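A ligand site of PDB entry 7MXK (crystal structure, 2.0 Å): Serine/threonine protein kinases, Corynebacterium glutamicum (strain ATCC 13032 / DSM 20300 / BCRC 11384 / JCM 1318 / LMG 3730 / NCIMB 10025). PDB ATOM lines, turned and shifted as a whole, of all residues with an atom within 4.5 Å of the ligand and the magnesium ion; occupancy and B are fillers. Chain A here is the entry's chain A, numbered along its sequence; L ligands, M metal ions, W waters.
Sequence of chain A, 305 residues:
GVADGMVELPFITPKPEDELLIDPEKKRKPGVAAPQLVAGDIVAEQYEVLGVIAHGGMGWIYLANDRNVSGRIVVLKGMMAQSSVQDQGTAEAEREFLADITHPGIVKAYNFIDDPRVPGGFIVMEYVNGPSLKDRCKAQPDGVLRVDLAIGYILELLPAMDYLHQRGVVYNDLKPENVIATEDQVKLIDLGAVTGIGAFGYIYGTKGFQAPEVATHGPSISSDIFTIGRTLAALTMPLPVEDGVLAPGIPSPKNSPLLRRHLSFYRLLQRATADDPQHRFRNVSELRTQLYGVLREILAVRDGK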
ATOM      1  N   ILE A  53      -3.750  -4.248 -25.638  1.00  0.00           N
ATOM      2  CA  ILE A  53      -4.170  -3.561 -24.427  1.00  0.00           C
ATOM      3  C   ILE A  53      -4.745  -4.507 -23.381  1.00  0.00           C
ATOM      4  O   ILE A  53      -4.809  -4.127 -22.203  1.00  0.00           O
ATOM      5  CB  ILE A  53      -5.192  -2.445 -24.751  1.00  0.00           C
ATOM      6  CG1 ILE A  53      -6.444  -3.051 -25.399  1.00  0.00           C
ATOM      7  CG2 ILE A  53      -4.572  -1.407 -25.670  1.00  0.00           C
ATOM      8  CD1 ILE A  53      -7.522  -2.036 -25.721  1.00  0.00           C
ATOM      9  N   ALA A  54      -5.165  -5.709 -23.771  1.00  0.00           N
ATOM     10  CA  ALA A  54      -5.719  -6.685 -22.842  1.00  0.00           C
ATOM     11  C   ALA A  54      -5.811  -8.030 -23.552  1.00  0.00           C
ATOM     12  O   ALA A  54      -5.845  -8.094 -24.781  1.00  0.00           O
ATOM     13  CB  ALA A  54      -7.085  -6.272 -22.301  1.00  0.00           C
ATOM     14  N   GLY A  56      -8.538 -10.963 -23.444  1.00  0.00           N
ATOM     15  CA  GLY A  56      -9.859 -11.324 -22.998  1.00  0.00           C
ATOM     16  C   GLY A  56     -10.203 -12.769 -23.297  1.00  0.00           C
ATOM     17  O   GLY A  56      -9.389 -13.554 -23.803  1.00  0.00           O
ATOM     18  N   GLY A  57     -11.452 -13.128 -22.990  1.00  0.00           N
ATOM     19  CA  GLY A  57     -11.925 -14.474 -23.267  1.00  0.00           C
ATOM     20  C   GLY A  57     -12.019 -14.800 -24.745  1.00  0.00           C
ATOM     21  O   GLY A  57     -11.986 -15.979 -25.105  1.00  0.00           O
ATOM     22  N   MET A  58     -12.131 -13.798 -25.602  1.00  0.00           N
ATOM     23  CA  MET A  58     -12.215 -13.984 -27.047  1.00  0.00           C
ATOM     24  C   MET A  58     -10.874 -13.764 -27.745  1.00  0.00           C
ATOM     25  O   MET A  58     -10.817 -13.794 -28.980  1.00  0.00           O
ATOM     26  CB  MET A  58     -13.278 -13.061 -27.643  1.00  0.00           C
ATOM     27  CG  MET A  58     -14.675 -13.269 -27.035  1.00  0.00           C
ATOM     28  SD  MET A  58     -15.949 -12.177 -27.714  1.00  0.00           S
ATOM     29  CE  MET A  58     -15.219 -10.578 -27.439  1.00  0.00           C
ATOM     30  N   GLY A  59      -9.797 -13.540 -26.997  1.00  0.00           N
ATOM     31  CA  GLY A  59      -8.466 -13.391 -27.552  1.00  0.00           C
ATOM     32  C   GLY A  59      -7.856 -12.044 -27.210  1.00  0.00           C
ATOM     33  O   GLY A  59      -8.373 -11.273 -26.393  1.00  0.00           O
ATOM     34  N   ILE A  61      -6.615  -8.154 -27.666  1.00  0.00           N
ATOM     35  CA  ILE A  61      -7.316  -6.934 -28.070  1.00  0.00           C
ATOM     36  C   ILE A  61      -6.251  -5.895 -28.435  1.00  0.00           C
ATOM     37  O   ILE A  61      -5.428  -5.519 -27.592  1.00  0.00           O
ATOM     38  CB  ILE A  61      -8.249  -6.431 -26.958  1.00  0.00           C
ATOM     39  CG1 ILE A  61      -9.271  -7.520 -26.606  1.00  0.00           C
ATOM     40  CG2 ILE A  61      -8.956  -5.163 -27.383  1.00  0.00           C
ATOM     41  CD1 ILE A  61     -10.206  -7.134 -25.494  1.00  0.00           C
ATOM     42  N   VAL A  75      -9.387   0.497 -31.670  1.00  0.00           N
ATOM     43  CA  VAL A  75      -9.282  -0.826 -31.074  1.00  0.00           C
ATOM     44  C   VAL A  75      -9.699  -1.859 -32.106  1.00  0.00           C
ATOM     45  O   VAL A  75     -10.680  -1.665 -32.843  1.00  0.00           O
ATOM     46  CB  VAL A  75     -10.160  -0.929 -29.806  1.00  0.00           C
ATOM     47  CG1 VAL A  75     -10.317  -2.375 -29.374  1.00  0.00           C
ATOM     48  CG2 VAL A  75      -9.574  -0.094 -28.683  1.00  0.00           C
ATOM     49  N   LYS A  77     -10.979  -5.517 -31.996  1.00  0.00           N
ATOM     50  CA  LYS A  77     -11.509  -6.537 -31.102  1.00  0.00           C
ATOM     51  C   LYS A  77     -12.099  -7.679 -31.924  1.00  0.00           C
ATOM     52  O   LYS A  77     -12.712  -7.447 -32.965  1.00  0.00           O
ATOM     53  CB  LYS A  77     -12.566  -5.965 -30.163  1.00  0.00           C
ATOM     54  CG  LYS A  77     -13.078  -6.951 -29.123  1.00  0.00           C
ATOM     55  CD  LYS A  77     -14.053  -6.292 -28.168  1.00  0.00           C
ATOM     56  CE  LYS A  77     -14.368  -7.190 -26.985  1.00  0.00           C
ATOM     57  NZ  LYS A  77     -15.460  -6.631 -26.160  1.00  0.00           N
ATOM     58  N   VAL A 107     -19.588   3.120 -27.132  1.00  0.00           N
ATOM     59  CA  VAL A 107     -18.408   3.195 -27.986  1.00  0.00           C
ATOM     60  C   VAL A 107     -18.828   3.143 -29.453  1.00  0.00           C
ATOM     61  O   VAL A 107     -19.811   2.494 -29.815  1.00  0.00           O
ATOM     62  CB  VAL A 107     -17.430   2.054 -27.640  1.00  0.00           C
ATOM     63  CG1 VAL A 107     -17.937   0.703 -28.153  1.00  0.00           C
ATOM     64  CG2 VAL A 107     -16.048   2.356 -28.189  1.00  0.00           C
ATOM     65  N   MET A 125     -13.256  -0.215 -33.477  1.00  0.00           N
ATOM     66  CA  MET A 125     -14.053   0.645 -32.623  1.00  0.00           C
ATOM     67  C   MET A 125     -13.182   1.691 -31.944  1.00  0.00           C
ATOM     68  O   MET A 125     -11.950   1.596 -31.897  1.00  0.00           O
ATOM     69  CB  MET A 125     -14.807  -0.161 -31.554  1.00  0.00           C
ATOM     70  CG  MET A 125     -13.936  -0.782 -30.486  1.00  0.00           C
ATOM     71  SD  MET A 125     -14.892  -1.729 -29.283  1.00  0.00           S
ATOM     72  CE  MET A 125     -15.636  -2.982 -30.322  1.00  0.00           C
ATOM     73  N   GLU A 126     -13.857   2.711 -31.423  1.00  0.00           N
ATOM     74  CA  GLU A 126     -13.210   3.786 -30.683  1.00  0.00           C
ATOM     75  C   GLU A 126     -12.503   3.236 -29.461  1.00  0.00           C
ATOM     76  O   GLU A 126     -12.992   2.322 -28.785  1.00  0.00           O
ATOM     77  CB  GLU A 126     -14.269   4.820 -30.286  1.00  0.00           C
ATOM     78  CG  GLU A 126     -13.861   5.863 -29.256  1.00  0.00           C
ATOM     79  CD  GLU A 126     -15.066   6.536 -28.623  1.00  0.00           C
ATOM     80  OE1 GLU A 126     -16.211   6.144 -28.934  1.00  0.00           O
ATOM     81  OE2 GLU A 126     -14.876   7.451 -27.797  1.00  0.00           O
ATOM     82  N   TYR A 127     -11.328   3.787 -29.168  1.00  0.00           N
ATOM     83  CA  TYR A 127     -10.602   3.456 -27.951  1.00  0.00           C
ATOM     84  C   TYR A 127     -11.093   4.337 -26.810  1.00  0.00           C
ATOM     85  O   TYR A 127     -11.184   5.565 -26.973  1.00  0.00           O
ATOM     86  CB  TYR A 127      -9.088   3.632 -28.149  1.00  0.00           C
ATOM     87  CG  TYR A 127      -8.282   3.468 -26.883  1.00  0.00           C
ATOM     88  CD1 TYR A 127      -8.108   2.216 -26.298  1.00  0.00           C
ATOM     89  CD2 TYR A 127      -7.691   4.568 -26.263  1.00  0.00           C
ATOM     90  CE1 TYR A 127      -7.373   2.066 -25.138  1.00  0.00           C
ATOM     91  CE2 TYR A 127      -6.949   4.424 -25.103  1.00  0.00           C
ATOM     92  CZ  TYR A 127      -6.797   3.166 -24.548  1.00  0.00           C
ATOM     93  OH  TYR A 127      -6.063   3.015 -23.388  1.00  0.00           O
ATOM     94  N   VAL A 128     -11.417   3.730 -25.677  1.00  0.00           N
ATOM     95  CA  VAL A 128     -11.850   4.461 -24.486  1.00  0.00           C
ATOM     96  C   VAL A 128     -10.746   4.357 -23.438  1.00  0.00           C
ATOM     97  O   VAL A 128     -10.351   3.253 -23.045  1.00  0.00           O
ATOM     98  CB  VAL A 128     -13.185   3.940 -23.943  1.00  0.00           C
ATOM     99  CG1 VAL A 128     -13.753   4.916 -22.911  1.00  0.00           C
ATOM    100  CG2 VAL A 128     -14.167   3.725 -25.079  1.00  0.00           C
ATOM    101  N   SER A 132     -11.961   0.255 -16.355  1.00  0.00           N
ATOM    102  CA  SER A 132     -13.273  -0.348 -16.286  1.00  0.00           C
ATOM    103  C   SER A 132     -13.794  -0.329 -14.856  1.00  0.00           C
ATOM    104  O   SER A 132     -13.050  -0.113 -13.904  1.00  0.00           O
ATOM    105  CB  SER A 132     -13.242  -1.790 -16.814  1.00  0.00           C
ATOM    106  OG  SER A 132     -12.710  -2.668 -15.840  1.00  0.00           O
ATOM    107  N   ASP A 173     -24.576  -8.170 -22.568  1.00  0.00           N
ATOM    108  CA  ASP A 173     -23.402  -8.609 -21.819  1.00  0.00           C
ATOM    109  C   ASP A 173     -22.926  -7.583 -20.797  1.00  0.00           C
ATOM    110  O   ASP A 173     -21.731  -7.487 -20.511  1.00  0.00           O
ATOM    111  CB  ASP A 173     -22.253  -8.983 -22.762  1.00  0.00           C
ATOM    112  CG  ASP A 173     -21.198  -9.862 -22.087  1.00  0.00           C
ATOM    113  OD1 ASP A 173     -21.510 -10.472 -21.038  1.00  0.00           O
ATOM    114  OD2 ASP A 173     -20.049  -9.926 -22.583  1.00  0.00           O
ATOM    115  N   LYS A 175     -21.618  -5.995 -17.647  1.00  0.00           N
ATOM    116  CA  LYS A 175     -20.879  -6.449 -16.478  1.00  0.00           C
ATOM    117  C   LYS A 175     -19.759  -5.435 -16.231  1.00  0.00           C
ATOM    118  O   LYS A 175     -19.385  -4.707 -17.148  1.00  0.00           O
ATOM    119  CB  LYS A 175     -20.305  -7.861 -16.679  1.00  0.00           C
ATOM    120  CG  LYS A 175     -19.453  -8.028 -17.929  1.00  0.00           C
ATOM    121  CD  LYS A 175     -18.873  -9.425 -18.023  1.00  0.00           C
ATOM    122  CE  LYS A 175     -18.180  -9.645 -19.355  1.00  0.00           C
ATOM    123  NZ  LYS A 175     -17.677 -11.036 -19.505  1.00  0.00           N
ATOM    124  N   GLU A 177     -16.659  -5.230 -16.240  1.00  0.00           N
ATOM    125  CA  GLU A 177     -15.420  -5.155 -17.013  1.00  0.00           C
ATOM    126  C   GLU A 177     -15.601  -4.541 -18.397  1.00  0.00           C
ATOM    127  O   GLU A 177     -14.591  -4.205 -19.029  1.00  0.00           O
ATOM    128  CB  GLU A 177     -14.771  -6.543 -17.140  1.00  0.00           C
ATOM    129  CG  GLU A 177     -15.401  -7.444 -18.186  1.00  0.00           C
ATOM    130  CD  GLU A 177     -14.834  -8.850 -18.152  1.00  0.00           C
ATOM    131  OE1 GLU A 177     -14.201  -9.194 -17.132  1.00  0.00           O
ATOM    132  OE2 GLU A 177     -15.019  -9.613 -19.126  1.00  0.00           O
ATOM    133  N   ASN A 178     -16.818  -4.386 -18.901  1.00  0.00           N
ATOM    134  CA  ASN A 178     -17.024  -3.707 -20.173  1.00  0.00           C
ATOM    135  C   ASN A 178     -17.808  -2.408 -20.021  1.00  0.00           C
ATOM    136  O   ASN A 178     -18.521  -1.982 -20.928  1.00  0.00           O
ATOM    137  CB  ASN A 178     -17.660  -4.632 -21.217  1.00  0.00           C
ATOM    138  CG  ASN A 178     -19.031  -5.165 -20.824  1.00  0.00           C
ATOM    139  OD1 ASN A 178     -19.860  -4.437 -20.291  1.00  0.00           O
ATOM    140  ND2 ASN A 178     -19.273  -6.439 -21.125  1.00  0.00           N
ATOM    141  N   ILE A 180     -16.457   1.381 -19.102  1.00  0.00           N
ATOM    142  CA  ILE A 180     -15.249   2.160 -18.892  1.00  0.00           C
ATOM    143  C   ILE A 180     -15.626   3.524 -18.332  1.00  0.00           C
ATOM    144  O   ILE A 180     -16.474   4.224 -18.902  1.00  0.00           O
ATOM    145  CB  ILE A 180     -14.442   2.310 -20.183  1.00  0.00           C
ATOM    146  CG1 ILE A 180     -14.063   0.942 -20.772  1.00  0.00           C
ATOM    147  CG2 ILE A 180     -13.197   3.140 -19.928  1.00  0.00           C
ATOM    148  CD1 ILE A 180     -13.048   0.176 -19.962  1.00  0.00           C
ATOM    149  N   ILE A 189     -18.758  -0.617 -23.842  1.00  0.00           N
ATOM    150  CA  ILE A 189     -17.766  -0.927 -24.867  1.00  0.00           C
ATOM    151  C   ILE A 189     -18.004  -2.258 -25.567  1.00  0.00           C
ATOM    152  O   ILE A 189     -17.283  -2.562 -26.530  1.00  0.00           O
ATOM    153  CB  ILE A 189     -16.329  -0.890 -24.303  1.00  0.00           C
ATOM    154  CG1 ILE A 189     -16.110  -2.017 -23.296  1.00  0.00           C
ATOM    155  CG2 ILE A 189     -16.053   0.456 -23.667  1.00  0.00           C
ATOM    156  CD1 ILE A 189     -14.682  -2.092 -22.776  1.00  0.00           C
ATOM    157  N   ASP A 190     -18.976  -3.069 -25.153  1.00  0.00           N
ATOM    158  CA  ASP A 190     -19.124  -4.405 -25.740  1.00  0.00           C
ATOM    159  C   ASP A 190     -20.125  -4.363 -26.902  1.00  0.00           C
ATOM    160  O   ASP A 190     -21.212  -4.948 -26.857  1.00  0.00           O
ATOM    161  CB  ASP A 190     -19.535  -5.412 -24.677  1.00  0.00           C
ATOM    162  CG  ASP A 190     -19.234  -6.848 -25.083  1.00  0.00           C
ATOM    163  OD1 ASP A 190     -18.816  -7.065 -26.238  1.00  0.00           O
ATOM    164  OD2 ASP A 190     -19.414  -7.750 -24.240  1.00  0.00           O
ATOM    165  N   TYR A 204     -24.189 -13.761 -26.670  1.00  0.00           N
ATOM    166  CA  TYR A 204     -22.891 -13.743 -25.990  1.00  0.00           C
ATOM    167  C   TYR A 204     -22.948 -12.931 -24.694  1.00  0.00           C
ATOM    168  O   TYR A 204     -22.233 -11.948 -24.495  1.00  0.00           O
ATOM    169  CB  TYR A 204     -21.810 -13.234 -26.932  1.00  0.00           C
ATOM    170  CG  TYR A 204     -21.524 -14.200 -28.046  1.00  0.00           C
ATOM    171  CD1 TYR A 204     -20.651 -15.264 -27.865  1.00  0.00           C
ATOM    172  CD2 TYR A 204     -22.154 -14.065 -29.283  1.00  0.00           C
ATOM    173  CE1 TYR A 204     -20.398 -16.159 -28.896  1.00  0.00           C
ATOM    174  CE2 TYR A 204     -21.894 -14.953 -30.315  1.00  0.00           C
ATOM    175  CZ  TYR A 204     -21.012 -15.996 -30.115  1.00  0.00           C
ATOM    176  OH  TYR A 204     -20.768 -16.881 -31.148  1.00  0.00           O
HETATM  177  P1  LIG L   1     -16.090 -11.507 -23.001  1.00  0.00           P
HETATM  178  O1  LIG L   1     -15.885 -12.964 -22.811  1.00  0.00           O
HETATM  179  O2  LIG L   1     -15.906 -10.703 -21.626  1.00  0.00           O
HETATM  180  O3  LIG L   1     -17.591 -11.261 -23.540  1.00  0.00           O
HETATM  181  P2  LIG L   1     -13.524 -10.469 -23.793  1.00  0.00           P
HETATM  182  O4  LIG L   1     -13.099 -10.877 -22.441  1.00  0.00           O
HETATM  183  O5  LIG L   1     -12.552 -11.120 -24.906  1.00  0.00           O
HETATM  184  N1  LIG L   1     -15.072 -10.893 -24.117  1.00  0.00           N
HETATM  185  P3  LIG L   1     -14.036  -7.729 -22.989  1.00  0.00           P
HETATM  186  O6  LIG L   1     -15.189  -7.069 -23.629  1.00  0.00           O
HETATM  187  O7  LIG L   1     -14.389  -8.245 -21.626  1.00  0.00           O
HETATM  188  O8  LIG L   1     -13.482  -8.880 -23.957  1.00  0.00           O
HETATM  189  O9  LIG L   1     -12.827  -6.683 -22.797  1.00  0.00           O
HETATM  190  C1  LIG L   1     -11.650  -7.036 -22.065  1.00  0.00           C
HETATM  191  C2  LIG L   1     -10.908  -5.759 -21.708  1.00  0.00           C
HETATM  192  O10 LIG L   1     -10.440  -5.138 -22.898  1.00  0.00           O
HETATM  193  C3  LIG L   1     -11.863  -4.724 -21.126  1.00  0.00           C
HETATM  194  O11 LIG L   1     -12.012  -4.880 -19.703  1.00  0.00           O
HETATM  195  C4  LIG L   1     -11.168  -3.405 -21.441  1.00  0.00           C
HETATM  196  O12 LIG L   1     -10.192  -3.130 -20.433  1.00  0.00           O
HETATM  197  C5  LIG L   1     -10.428  -3.720 -22.736  1.00  0.00           C
HETATM  198  N2  LIG L   1     -11.146  -3.109 -23.880  1.00  0.00           N
HETATM  199  C6  LIG L   1     -11.951  -3.759 -24.732  1.00  0.00           C
HETATM  200  N3  LIG L   1     -12.436  -2.885 -25.645  1.00  0.00           N
HETATM  201  C7  LIG L   1     -11.922  -1.673 -25.350  1.00  0.00           C
HETATM  202  C8  LIG L   1     -12.062  -0.327 -25.966  1.00  0.00           C
HETATM  203  N4  LIG L   1     -12.834  -0.131 -27.055  1.00  0.00           N
HETATM  204  N5  LIG L   1     -11.388   0.693 -25.395  1.00  0.00           N
HETATM  205  C9  LIG L   1     -10.633   0.439 -24.329  1.00  0.00           C
HETATM  206  N6  LIG L   1     -10.463  -0.747 -23.731  1.00  0.00           N
HETATM  207  C10 LIG L   1     -11.107  -1.826 -24.235  1.00  0.00           C
HETATM  208 MG1  LIG L   1     -14.089 -10.097 -20.996  1.00  0.00          MG
HETATM  209 MG    MG M   1     -18.688  -9.567 -23.861  1.00  0.00          MG
HETATM  210  O   HOH W   1      -7.980  -4.728 -19.024  1.00  0.00           O
HETATM  211  O   HOH W   2     -13.982 -12.091 -20.060  1.00  0.00           O
HETATM  212  O   HOH W   3     -11.042  -4.820 -16.864  1.00  0.00           O
HETATM  213  O   HOH W   4     -17.263  -8.443 -22.582  1.00  0.00           O
HETATM  214  O   HOH W   5     -14.985  -3.732 -26.653  1.00  0.00           O
HETATM  215  O   HOH W   6     -12.210  -9.701 -19.958  1.00  0.00           O
HETATM  216  O   HOH W   7     -19.903 -10.737 -25.001  1.00  0.00           O
HETATM  217  O   HOH W   8     -11.258 -10.220 -27.139  1.00  0.00           O
HETATM  218  O   HOH W   9      -9.603  -9.012 -20.534  1.00  0.00           O
HETATM  219  O   HOH W  10     -17.560  -9.257 -25.518  1.00  0.00           O
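O of Glu 126 is in hydrogen-bond range of N4 of the ligand, at 3.0 Å.
The side-chain amino group (NZ) of Lys 77 is in salt-bridge range of an oxygen (O6) of the ligand (2.6 Å).
A magnesium atom (MG1) of the ligand is bound by the side-chain carboxylate (OE2) of Glu 177.
N5 of the ligand is in hydrogen-bond range of N of Val 128.
An oxygen (O5) of the ligand lies within hydrogen-bond range of the backbone NH (N) of Gly 57.
O of Glu 177 is in hydrogen-bond range of O11 of the ligand (2.7 Å).
A nitrogen (N4) of the ligand is in hydrogen-bond range of the side-chain sulfur (SD) of Met 125 (3.4 Å).
The backbone NH (N) of Met 58 is in hydrogen-bond range of an oxygen (O5) of the ligand, at 2.8 Å.
OE2 of Glu 177 sits close to NZ of Lys 175, 3.0 Å away.
The backbone NH (N) of Ile 189 lies within hydrogen-bond range of the backbone carbonyl oxygen (O) of Asn 178 (3.2 Å).
The backbone NH (N) of Val 75 lies within hydrogen-bond range of the backbone carbonyl oxygen (O) of Met 125 (2.8 Å).
The backbone NH (N) of Ile 53 sits at hydrogen-bond distance from the backbone carbonyl oxygen (O) of Ile 61, at 2.9 Å.
The backbone carbonyl oxygen (O) of Lys 175 sits close to the side-chain amide oxygen (OD1) of Asn 178, 3.2 Å away.
O of Asp 173 lies within hydrogen-bond range of ND2 of Asn 178, at 2.7 Å.
The side-chain carboxylate (OD1) of Asp 190 lies within salt-bridge range of the side-chain amino group (NZ) of Lys 77, 3.4 Å away.
OD2 of Asp 190 sits close to ND2 of Asn 178, at 3.4 Å.
The side-chain amino group (NZ) of Lys 175 lies close to an oxygen (O2) of the ligand.
CD1 of Ile 53 touches N6 of the ligand, at 3.8 Å.
Ala 54 touches the ligand.
Gly 56 touches the ligand.
CD1 of Ile 61 touches O10 of the ligand, 3.3 Å away.
CG2 of Val 75 touches N4 of the ligand, at 3.6 Å.
Tyr 127 touches the ligand (CD1 to C9, 3.7 Å).
CD1 of Ile 189 touches N3 of the ligand, at 3.7 Å.
16 residues have an atom within 4 Å of the ligand: Ile 53, Ala 54, Gly 56, Gly 57, Met 58, Ile 61, Val 75, Lys 77, Met 125, Glu 126, Tyr 127, Val 128, Asp 173, Lys 175, Glu 177 and Ile 189.
Along chain A the residues within 4 Å of the ligand span positions 53 to 189.
The magnesium ion is bound by OD2 of Asp 173 (1.9 Å), OD2 of Asp 190 (2.0 Å), water W10 (2.0 Å), water W7 (2.0 Å), O3 of the ligand (2.0 Å) and water W4 (2.2 Å).
The magnesium ion has six donor atoms within binding distance.
Water W10 lies within hydrogen-bond range of OD1 of Asp 190 (2.6 Å), N1 of the ligand (3.3 Å) and NZ of Lys 77 (3.4 Å).
Water W4 lies within hydrogen-bond range of an oxygen (O6) of the ligand (2.7 Å) and the side-chain amide nitrogen (ND2) of Asn 178 (3.2 Å).
Water W8 bridges O5 of the ligand (2.7 Å) and O of Gly 59 (3.2 Å).
Water W3 bridges the side-chain hydroxyl of Ser 132 (2.9 Å) and an oxygen (O11) of the ligand (3.0 Å).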
